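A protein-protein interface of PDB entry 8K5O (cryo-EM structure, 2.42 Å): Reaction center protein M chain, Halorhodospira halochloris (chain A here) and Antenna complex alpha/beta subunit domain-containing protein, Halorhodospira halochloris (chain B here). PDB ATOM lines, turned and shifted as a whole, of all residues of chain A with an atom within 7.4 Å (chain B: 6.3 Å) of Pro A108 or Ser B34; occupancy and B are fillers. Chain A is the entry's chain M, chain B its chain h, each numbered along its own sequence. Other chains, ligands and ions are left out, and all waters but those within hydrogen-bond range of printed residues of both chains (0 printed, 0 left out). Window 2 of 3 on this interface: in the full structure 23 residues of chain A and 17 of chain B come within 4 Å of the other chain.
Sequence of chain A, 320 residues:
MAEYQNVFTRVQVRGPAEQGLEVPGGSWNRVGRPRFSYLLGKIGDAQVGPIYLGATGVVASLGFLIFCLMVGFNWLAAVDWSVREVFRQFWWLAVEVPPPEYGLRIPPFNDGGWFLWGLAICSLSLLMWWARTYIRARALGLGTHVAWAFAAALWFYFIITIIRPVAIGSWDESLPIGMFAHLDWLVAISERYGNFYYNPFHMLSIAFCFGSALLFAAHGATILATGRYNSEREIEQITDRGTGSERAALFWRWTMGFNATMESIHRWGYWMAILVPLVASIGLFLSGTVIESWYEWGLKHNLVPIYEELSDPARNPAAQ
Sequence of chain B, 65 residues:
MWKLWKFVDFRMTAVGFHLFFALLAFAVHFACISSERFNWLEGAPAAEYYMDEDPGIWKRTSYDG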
ATOM      1  N   PRO A  98      13.466  14.641  -0.262  1.00  0.00           N
ATOM      2  CA  PRO A  98      13.926  14.694   1.121  1.00  0.00           C
ATOM      3  C   PRO A  98      12.970  13.953   2.036  1.00  0.00           C
ATOM      4  O   PRO A  98      11.752  13.909   1.785  1.00  0.00           O
ATOM      5  CB  PRO A  98      13.942  16.196   1.429  1.00  0.00           C
ATOM      6  CG  PRO A  98      14.058  16.846   0.117  1.00  0.00           C
ATOM      7  CD  PRO A  98      13.299  15.989  -0.830  1.00  0.00           C
ATOM      8  N   PRO A  99      13.478  13.364   3.111  1.00  0.00           N
ATOM      9  CA  PRO A  99      12.607  12.712   4.085  1.00  0.00           C
ATOM     10  C   PRO A  99      11.842  13.741   4.898  1.00  0.00           C
ATOM     11  O   PRO A  99      12.187  14.931   4.888  1.00  0.00           O
ATOM     12  CB  PRO A  99      13.587  11.919   4.965  1.00  0.00           C
ATOM     13  CG  PRO A  99      14.905  12.023   4.316  1.00  0.00           C
ATOM     14  CD  PRO A  99      14.892  13.239   3.477  1.00  0.00           C
ATOM     15  N   TYR A 102      13.217  16.806   7.429  1.00  0.00           N
ATOM     16  CA  TYR A 102      13.638  18.133   7.001  1.00  0.00           C
ATOM     17  C   TYR A 102      12.474  19.097   6.858  1.00  0.00           C
ATOM     18  O   TYR A 102      12.678  20.310   6.972  1.00  0.00           O
ATOM     19  CB  TYR A 102      14.393  18.052   5.677  1.00  0.00           C
ATOM     20  CG  TYR A 102      15.701  17.319   5.785  1.00  0.00           C
ATOM     21  CD1 TYR A 102      16.835  17.958   6.256  1.00  0.00           C
ATOM     22  CD2 TYR A 102      15.798  15.986   5.430  1.00  0.00           C
ATOM     23  CE1 TYR A 102      18.029  17.291   6.366  1.00  0.00           C
ATOM     24  CE2 TYR A 102      16.985  15.314   5.534  1.00  0.00           C
ATOM     25  CZ  TYR A 102      18.101  15.968   6.001  1.00  0.00           C
ATOM     26  OH  TYR A 102      19.295  15.297   6.107  1.00  0.00           O
ATOM     27  N   ARG A 105      13.074  22.224   4.744  1.00  0.00           N
ATOM     28  CA  ARG A 105      14.501  22.482   4.621  1.00  0.00           C
ATOM     29  C   ARG A 105      15.057  21.800   3.381  1.00  0.00           C
ATOM     30  O   ARG A 105      14.681  20.673   3.051  1.00  0.00           O
ATOM     31  CB  ARG A 105      15.247  21.983   5.858  1.00  0.00           C
ATOM     32  CG  ARG A 105      14.979  22.766   7.119  1.00  0.00           C
ATOM     33  CD  ARG A 105      15.237  21.940   8.363  1.00  0.00           C
ATOM     34  NE  ARG A 105      16.572  21.360   8.380  1.00  0.00           N
ATOM     35  CZ  ARG A 105      16.867  20.176   8.897  1.00  0.00           C
ATOM     36  NH1 ARG A 105      15.936  19.406   9.433  1.00  0.00           N
ATOM     37  NH2 ARG A 105      18.127  19.754   8.876  1.00  0.00           N
ATOM     38  N   ILE A 106      15.958  22.490   2.692  1.00  0.00           N
ATOM     39  CA  ILE A 106      16.725  21.849   1.631  1.00  0.00           C
ATOM     40  C   ILE A 106      17.789  21.004   2.318  1.00  0.00           C
ATOM     41  O   ILE A 106      18.643  21.540   3.037  1.00  0.00           O
ATOM     42  CB  ILE A 106      17.344  22.868   0.663  1.00  0.00           C
ATOM     43  CG1 ILE A 106      16.261  23.675  -0.057  1.00  0.00           C
ATOM     44  CG2 ILE A 106      18.238  22.164  -0.342  1.00  0.00           C
ATOM     45  CD1 ILE A 106      15.914  24.980   0.616  1.00  0.00           C
ATOM     46  N   PRO A 107      17.771  19.689   2.134  1.00  0.00           N
ATOM     47  CA  PRO A 107      18.666  18.817   2.883  1.00  0.00           C
ATOM     48  C   PRO A 107      19.998  18.664   2.173  1.00  0.00           C
ATOM     49  O   PRO A 107      20.208  19.251   1.102  1.00  0.00           O
ATOM     50  CB  PRO A 107      17.894  17.494   2.910  1.00  0.00           C
ATOM     51  CG  PRO A 107      17.159  17.504   1.658  1.00  0.00           C
ATOM     52  CD  PRO A 107      16.817  18.919   1.322  1.00  0.00           C
ATOM     53  N   PRO A 108      20.931  17.898   2.741  1.00  0.00           N
ATOM     54  CA  PRO A 108      22.138  17.545   1.990  1.00  0.00           C
ATOM     55  C   PRO A 108      21.780  16.796   0.718  1.00  0.00           C
ATOM     56  O   PRO A 108      20.695  16.229   0.590  1.00  0.00           O
ATOM     57  CB  PRO A 108      22.915  16.657   2.963  1.00  0.00           C
ATOM     58  CG  PRO A 108      22.467  17.087   4.296  1.00  0.00           C
ATOM     59  CD  PRO A 108      21.033  17.490   4.153  1.00  0.00           C
ATOM     60  N   PHE A 109      22.719  16.799  -0.234  1.00  0.00           N
ATOM     61  CA  PHE A 109      22.438  16.247  -1.556  1.00  0.00           C
ATOM     62  C   PHE A 109      21.860  14.843  -1.487  1.00  0.00           C
ATOM     63  O   PHE A 109      20.836  14.556  -2.116  1.00  0.00           O
ATOM     64  CB  PHE A 109      23.693  16.210  -2.420  1.00  0.00           C
ATOM     65  CG  PHE A 109      24.089  17.522  -2.994  1.00  0.00           C
ATOM     66  CD1 PHE A 109      23.336  18.096  -3.997  1.00  0.00           C
ATOM     67  CD2 PHE A 109      25.279  18.114  -2.636  1.00  0.00           C
ATOM     68  CE1 PHE A 109      23.716  19.274  -4.569  1.00  0.00           C
ATOM     69  CE2 PHE A 109      25.665  19.294  -3.209  1.00  0.00           C
ATOM     70  CZ  PHE A 109      24.886  19.869  -4.180  1.00  0.00           C
ATOM     71  N   ASN A 110      22.504  14.008  -0.712  1.00  0.00           N
ATOM     72  CA  ASN A 110      22.104  12.630  -0.672  1.00  0.00           C
ATOM     73  C   ASN A 110      20.959  12.329   0.297  1.00  0.00           C
ATOM     74  O   ASN A 110      20.534  11.209   0.421  1.00  0.00           O
ATOM     75  CB  ASN A 110      23.376  11.801  -0.506  1.00  0.00           C
ATOM     76  CG  ASN A 110      23.749  11.051  -1.741  1.00  0.00           C
ATOM     77  OD1 ASN A 110      23.097  11.167  -2.762  1.00  0.00           O
ATOM     78  ND2 ASN A 110      24.779  10.250  -1.645  1.00  0.00           N
ATOM     79  N   ASP A 111      20.424  13.322   0.942  1.00  0.00           N
ATOM     80  CA  ASP A 111      19.238  13.160   1.772  1.00  0.00           C
ATOM     81  C   ASP A 111      18.048  13.887   1.167  1.00  0.00           C
ATOM     82  O   ASP A 111      17.213  14.439   1.879  1.00  0.00           O
ATOM     83  CB  ASP A 111      19.519  13.643   3.187  1.00  0.00           C
ATOM     84  CG  ASP A 111      18.802  12.822   4.229  1.00  0.00           C
ATOM     85  OD1 ASP A 111      18.061  11.897   3.845  1.00  0.00           O
ATOM     86  OD2 ASP A 111      19.004  13.075   5.432  1.00  0.00           O
ATOM     87  N   GLY A 112      17.954  13.894  -0.160  1.00  0.00           N
ATOM     88  CA  GLY A 112      16.921  14.616  -0.863  1.00  0.00           C
ATOM     89  C   GLY A 112      17.337  15.971  -1.387  1.00  0.00           C
ATOM     90  O   GLY A 112      16.546  16.617  -2.084  1.00  0.00           O
ATOM     91  N   GLY A 113      18.550  16.424  -1.069  1.00  0.00           N
ATOM     92  CA  GLY A 113      19.025  17.682  -1.613  1.00  0.00           C
ATOM     93  C   GLY A 113      19.226  17.629  -3.113  1.00  0.00           C
ATOM     94  O   GLY A 113      18.992  18.615  -3.811  1.00  0.00           O
ATOM     95  N   TRP A 114      19.675  16.484  -3.629  1.00  0.00           N
ATOM     96  CA  TRP A 114      19.785  16.338  -5.075  1.00  0.00           C
ATOM     97  C   TRP A 114      18.421  16.446  -5.728  1.00  0.00           C
ATOM     98  O   TRP A 114      18.294  16.995  -6.825  1.00  0.00           O
ATOM     99  CB  TRP A 114      20.436  15.005  -5.442  1.00  0.00           C
ATOM    100  CG  TRP A 114      21.914  15.072  -5.550  1.00  0.00           C
ATOM    101  CD1 TRP A 114      22.808  14.259  -4.937  1.00  0.00           C
ATOM    102  CD2 TRP A 114      22.678  16.005  -6.320  1.00  0.00           C
ATOM    103  NE1 TRP A 114      24.085  14.625  -5.265  1.00  0.00           N
ATOM    104  CE2 TRP A 114      24.033  15.697  -6.114  1.00  0.00           C
ATOM    105  CE3 TRP A 114      22.348  17.080  -7.152  1.00  0.00           C
ATOM    106  CZ2 TRP A 114      25.059  16.418  -6.714  1.00  0.00           C
ATOM    107  CZ3 TRP A 114      23.365  17.790  -7.747  1.00  0.00           C
ATOM    108  CH2 TRP A 114      24.705  17.456  -7.526  1.00  0.00           C
ATOM    109  N   PHE A 115      17.388  15.920  -5.071  1.00  0.00           N
ATOM    110  CA  PHE A 115      16.047  16.044  -5.616  1.00  0.00           C
ATOM    111  C   PHE A 115      15.620  17.499  -5.710  1.00  0.00           C
ATOM    112  O   PHE A 115      15.023  17.908  -6.703  1.00  0.00           O
ATOM    113  CB  PHE A 115      15.038  15.277  -4.773  1.00  0.00           C
ATOM    114  CG  PHE A 115      13.634  15.663  -5.075  1.00  0.00           C
ATOM    115  CD1 PHE A 115      13.041  15.246  -6.246  1.00  0.00           C
ATOM    116  CD2 PHE A 115      12.929  16.498  -4.232  1.00  0.00           C
ATOM    117  CE1 PHE A 115      11.771  15.623  -6.552  1.00  0.00           C
ATOM    118  CE2 PHE A 115      11.651  16.876  -4.540  1.00  0.00           C
ATOM    119  CZ  PHE A 115      11.073  16.433  -5.701  1.00  0.00           C
ATOM    120  N   LEU A 116      15.892  18.289  -4.673  1.00  0.00           N
ATOM    121  CA  LEU A 116      15.495  19.693  -4.697  1.00  0.00           C
ATOM    122  C   LEU A 116      16.324  20.483  -5.699  1.00  0.00           C
ATOM    123  O   LEU A 116      15.812  21.387  -6.364  1.00  0.00           O
ATOM    124  CB  LEU A 116      15.620  20.289  -3.299  1.00  0.00           C
ATOM    125  CG  LEU A 116      14.555  19.797  -2.324  1.00  0.00           C
ATOM    126  CD1 LEU A 116      14.598  20.603  -1.055  1.00  0.00           C
ATOM    127  CD2 LEU A 116      13.186  19.881  -2.967  1.00  0.00           C
ATOM    128  N   TRP A 117      17.610  20.154  -5.807  1.00  0.00           N
ATOM    129  CA  TRP A 117      18.470  20.738  -6.827  1.00  0.00           C
ATOM    130  C   TRP A 117      17.917  20.472  -8.220  1.00  0.00           C
ATOM    131  O   TRP A 117      17.762  21.390  -9.036  1.00  0.00           O
ATOM    132  CB  TRP A 117      19.874  20.151  -6.672  1.00  0.00           C
ATOM    133  CG  TRP A 117      20.931  20.776  -7.503  1.00  0.00           C
ATOM    134  CD1 TRP A 117      21.846  21.695  -7.095  1.00  0.00           C
ATOM    135  CD2 TRP A 117      21.204  20.519  -8.882  1.00  0.00           C
ATOM    136  NE1 TRP A 117      22.669  22.034  -8.135  1.00  0.00           N
ATOM    137  CE2 TRP A 117      22.294  21.326  -9.245  1.00  0.00           C
ATOM    138  CE3 TRP A 117      20.627  19.689  -9.848  1.00  0.00           C
ATOM    139  CZ2 TRP A 117      22.821  21.329 -10.528  1.00  0.00           C
ATOM    140  CZ3 TRP A 117      21.152  19.693 -11.118  1.00  0.00           C
ATOM    141  CH2 TRP A 117      22.233  20.511 -11.449  1.00  0.00           C
ATOM    142  N   HIS B  29      23.532  27.922  -5.538  1.00  0.00           N
ATOM    143  CA  HIS B  29      22.993  28.224  -4.218  1.00  0.00           C
ATOM    144  C   HIS B  29      22.430  26.973  -3.559  1.00  0.00           C
ATOM    145  O   HIS B  29      22.646  26.740  -2.365  1.00  0.00           O
ATOM    146  CB  HIS B  29      21.916  29.303  -4.327  1.00  0.00           C
ATOM    147  CG  HIS B  29      22.452  30.695  -4.469  1.00  0.00           C
ATOM    148  ND1 HIS B  29      22.674  31.288  -5.692  1.00  0.00           N
ATOM    149  CD2 HIS B  29      22.782  31.620  -3.540  1.00  0.00           C
ATOM    150  CE1 HIS B  29      23.120  32.518  -5.508  1.00  0.00           C
ATOM    151  NE2 HIS B  29      23.204  32.741  -4.210  1.00  0.00           N
ATOM    152  N   PHE B  30      21.714  26.147  -4.327  1.00  0.00           N
ATOM    153  CA  PHE B  30      21.194  24.893  -3.803  1.00  0.00           C
ATOM    154  C   PHE B  30      22.314  23.931  -3.448  1.00  0.00           C
ATOM    155  O   PHE B  30      22.189  23.168  -2.487  1.00  0.00           O
ATOM    156  CB  PHE B  30      20.253  24.253  -4.822  1.00  0.00           C
ATOM    157  CG  PHE B  30      18.836  24.724  -4.715  1.00  0.00           C
ATOM    158  CD1 PHE B  30      18.533  26.073  -4.782  1.00  0.00           C
ATOM    159  CD2 PHE B  30      17.803  23.820  -4.545  1.00  0.00           C
ATOM    160  CE1 PHE B  30      17.232  26.509  -4.689  1.00  0.00           C
ATOM    161  CE2 PHE B  30      16.498  24.253  -4.449  1.00  0.00           C
ATOM    162  CZ  PHE B  30      16.212  25.598  -4.521  1.00  0.00           C
ATOM    163  N   ALA B  31      23.405  23.947  -4.214  1.00  0.00           N
ATOM    164  CA  ALA B  31      24.569  23.143  -3.868  1.00  0.00           C
ATOM    165  C   ALA B  31      25.162  23.580  -2.537  1.00  0.00           C
ATOM    166  O   ALA B  31      25.579  22.744  -1.728  1.00  0.00           O
ATOM    167  CB  ALA B  31      25.614  23.232  -4.979  1.00  0.00           C
ATOM    168  N   CYS B  32      25.224  24.889  -2.304  1.00  0.00           N
ATOM    169  CA  CYS B  32      25.735  25.396  -1.036  1.00  0.00           C
ATOM    170  C   CYS B  32      24.820  25.017   0.121  1.00  0.00           C
ATOM    171  O   CYS B  32      25.298  24.633   1.193  1.00  0.00           O
ATOM    172  CB  CYS B  32      25.907  26.908  -1.109  1.00  0.00           C
ATOM    173  SG  CYS B  32      26.939  27.421  -2.472  1.00  0.00           S
ATOM    174  N   ILE B  33      23.506  25.125  -0.077  1.00  0.00           N
ATOM    175  CA  ILE B  33      22.563  24.718   0.962  1.00  0.00           C
ATOM    176  C   ILE B  33      22.692  23.228   1.248  1.00  0.00           C
ATOM    177  O   ILE B  33      22.619  22.791   2.402  1.00  0.00           O
ATOM    178  CB  ILE B  33      21.124  25.090   0.567  1.00  0.00           C
ATOM    179  CG1 ILE B  33      21.022  26.580   0.279  1.00  0.00           C
ATOM    180  CG2 ILE B  33      20.163  24.719   1.673  1.00  0.00           C
ATOM    181  CD1 ILE B  33      19.759  26.987  -0.423  1.00  0.00           C
ATOM    182  N   SER B  34      22.884  22.424   0.206  1.00  0.00           N
ATOM    183  CA  SER B  34      23.038  20.987   0.370  1.00  0.00           C
ATOM    184  C   SER B  34      24.337  20.613   1.068  1.00  0.00           C
ATOM    185  O   SER B  34      24.513  19.446   1.425  1.00  0.00           O
ATOM    186  CB  SER B  34      22.959  20.300  -0.990  1.00  0.00           C
ATOM    187  OG  SER B  34      21.628  20.277  -1.470  1.00  0.00           O
ATOM    188  N   SER B  35      25.248  21.558   1.251  1.00  0.00           N
ATOM    189  CA  SER B  35      26.488  21.332   1.977  1.00  0.00           C
ATOM    190  C   SER B  35      26.309  21.812   3.409  1.00  0.00           C
ATOM    191  O   SER B  35      25.831  22.925   3.634  1.00  0.00           O
ATOM    192  CB  SER B  35      27.647  22.063   1.303  1.00  0.00           C
ATOM    193  OG  SER B  35      28.837  21.934   2.058  1.00  0.00           O
ATOM    194  N   GLU B  36      26.682  20.971   4.375  1.00  0.00           N
ATOM    195  CA  GLU B  36      26.598  21.381   5.773  1.00  0.00           C
ATOM    196  C   GLU B  36      27.490  22.580   6.053  1.00  0.00           C
ATOM    197  O   GLU B  36      27.080  23.525   6.736  1.00  0.00           O
ATOM    198  CB  GLU B  36      26.992  20.234   6.697  1.00  0.00           C
ATOM    199  CG  GLU B  36      26.906  20.633   8.153  1.00  0.00           C
ATOM    200  CD  GLU B  36      27.361  19.555   9.097  1.00  0.00           C
ATOM    201  OE1 GLU B  36      27.811  18.495   8.628  1.00  0.00           O
ATOM    202  OE2 GLU B  36      27.252  19.764  10.319  1.00  0.00           O
ATOM    203  N   ASN B  39      25.856  25.668   4.228  1.00  0.00           N
ATOM    204  CA  ASN B  39      24.442  25.973   4.413  1.00  0.00           C
ATOM    205  C   ASN B  39      24.326  27.095   5.433  1.00  0.00           C
ATOM    206  O   ASN B  39      24.326  26.874   6.643  1.00  0.00           O
ATOM    207  CB  ASN B  39      23.672  24.739   4.855  1.00  0.00           C
ATOM    208  CG  ASN B  39      22.203  24.848   4.566  1.00  0.00           C
ATOM    209  OD1 ASN B  39      21.695  25.931   4.308  1.00  0.00           O
ATOM    210  ND2 ASN B  39      21.509  23.726   4.607  1.00  0.00           N
ATOM    211  N   GLU B  42      20.994  26.781   7.485  1.00  0.00           N
ATOM    212  CA  GLU B  42      21.065  26.004   8.713  1.00  0.00           C
ATOM    213  C   GLU B  42      22.119  26.527   9.674  1.00  0.00           C
ATOM    214  O   GLU B  42      21.948  26.405  10.889  1.00  0.00           O
ATOM    215  CB  GLU B  42      21.331  24.533   8.397  1.00  0.00           C
ATOM    216  CG  GLU B  42      20.254  23.897   7.544  1.00  0.00           C
ATOM    217  CD  GLU B  42      20.055  22.427   7.843  1.00  0.00           C
ATOM    218  OE1 GLU B  42      21.011  21.779   8.316  1.00  0.00           O
ATOM    219  OE2 GLU B  42      18.946  21.914   7.590  1.00  0.00           O
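The guanidinium group of Arg A105 is in salt-bridge range of the side-chain carboxylate of Glu B42, at 2.6 Å. The backbone carbonyl oxygen (O) of Pro A107 is in hydrogen-bond range of the side-chain hydroxyl (OG) of Ser B34 (3.1 Å).
The backbone carbonyl oxygen (O) of Pro A108 sits at hydrogen-bond distance from the backbone NH (N) of Gly A113 (2.7 Å). N of Trp A114 is in hydrogen-bond range of O of Phe A109 (2.7 Å). The side-chain hydroxyl (OG) of Ser B34 is in hydrogen-bond range of the backbone carbonyl oxygen (O) of Phe B30, 3.1 Å away. The backbone NH (N) of Asn B39 is in hydrogen-bond range of the backbone carbonyl oxygen (O) of Cys B32 (3.3 Å). O of Ile B33 is in hydrogen-bond range of ND2 of Asn B39, 2.6 Å away. The side-chain amide oxygen (OD1) of Asn B39 sits at hydrogen-bond distance from the backbone NH (N) of Glu B42 (3.4 Å).
Among the printed residues, merely in contact across the chains: Pro A108 with Ser B34 (3.1 Å), Phe A109 with Ala B31 (3.3 Å), Leu A116 with Phe B30 (3.5 Å), Ile A106 with Ile B33 (3.5 Å), Phe A109 with Ser B34 (3.6 Å), Gly A113 with Ser B34 (3.7 Å), Trp A117 with Phe B30 (3.8 Å), Ile A106 with Asn B39 (3.9 Å) and Trp A117 with Ala B31 (3.98 Å).
Printed residues of chain B within 4 Å of Pro A108: Ser B34. Ser B34 touches just these residues of chain A: Pro A107, Pro A108, Phe A109 and Gly A113. Of the printed residues of chain B, Pro A107 touches Ser B34. Of the printed residues of chain A, Phe B30 touches Leu A116 and Trp A117. Of the printed residues of chain A, Asn B39 touches Ile A106. Asp A111 touches none of the printed residues of chain B. Phe A115 touches none of the printed residues of chain B. The nearest residue of chain B that does not touch Pro A108 is Ser B35 (5.1 Å). The nearest printed residue of chain A that does not touch Asn B39 is Pro A107 (5.8 Å).
Of the 16 printed residues of chain A, 8 touch a printed residue of chain B. Hydrophobic or aromatic side chains of chain A within 4 Å of the printed part of chain B: Ile A106, Pro A108, Phe A109 and Trp A117. Along chain A the printed residues that touch a printed residue of chain B span positions 105 to 117. Of the 10 printed residues of chain B, 6 touch a printed residue of chain A. Hydrophobic or aromatic side chains of chain B that line the printed part of chain A: Phe B30, Ala B31 and Ile B33. Among the printed residues, Asp or Glu carboxylates within 4 Å of a Lys or Arg side-chain nitrogen of the other chain: Arg A105 with Glu B42 (2.6 Å).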
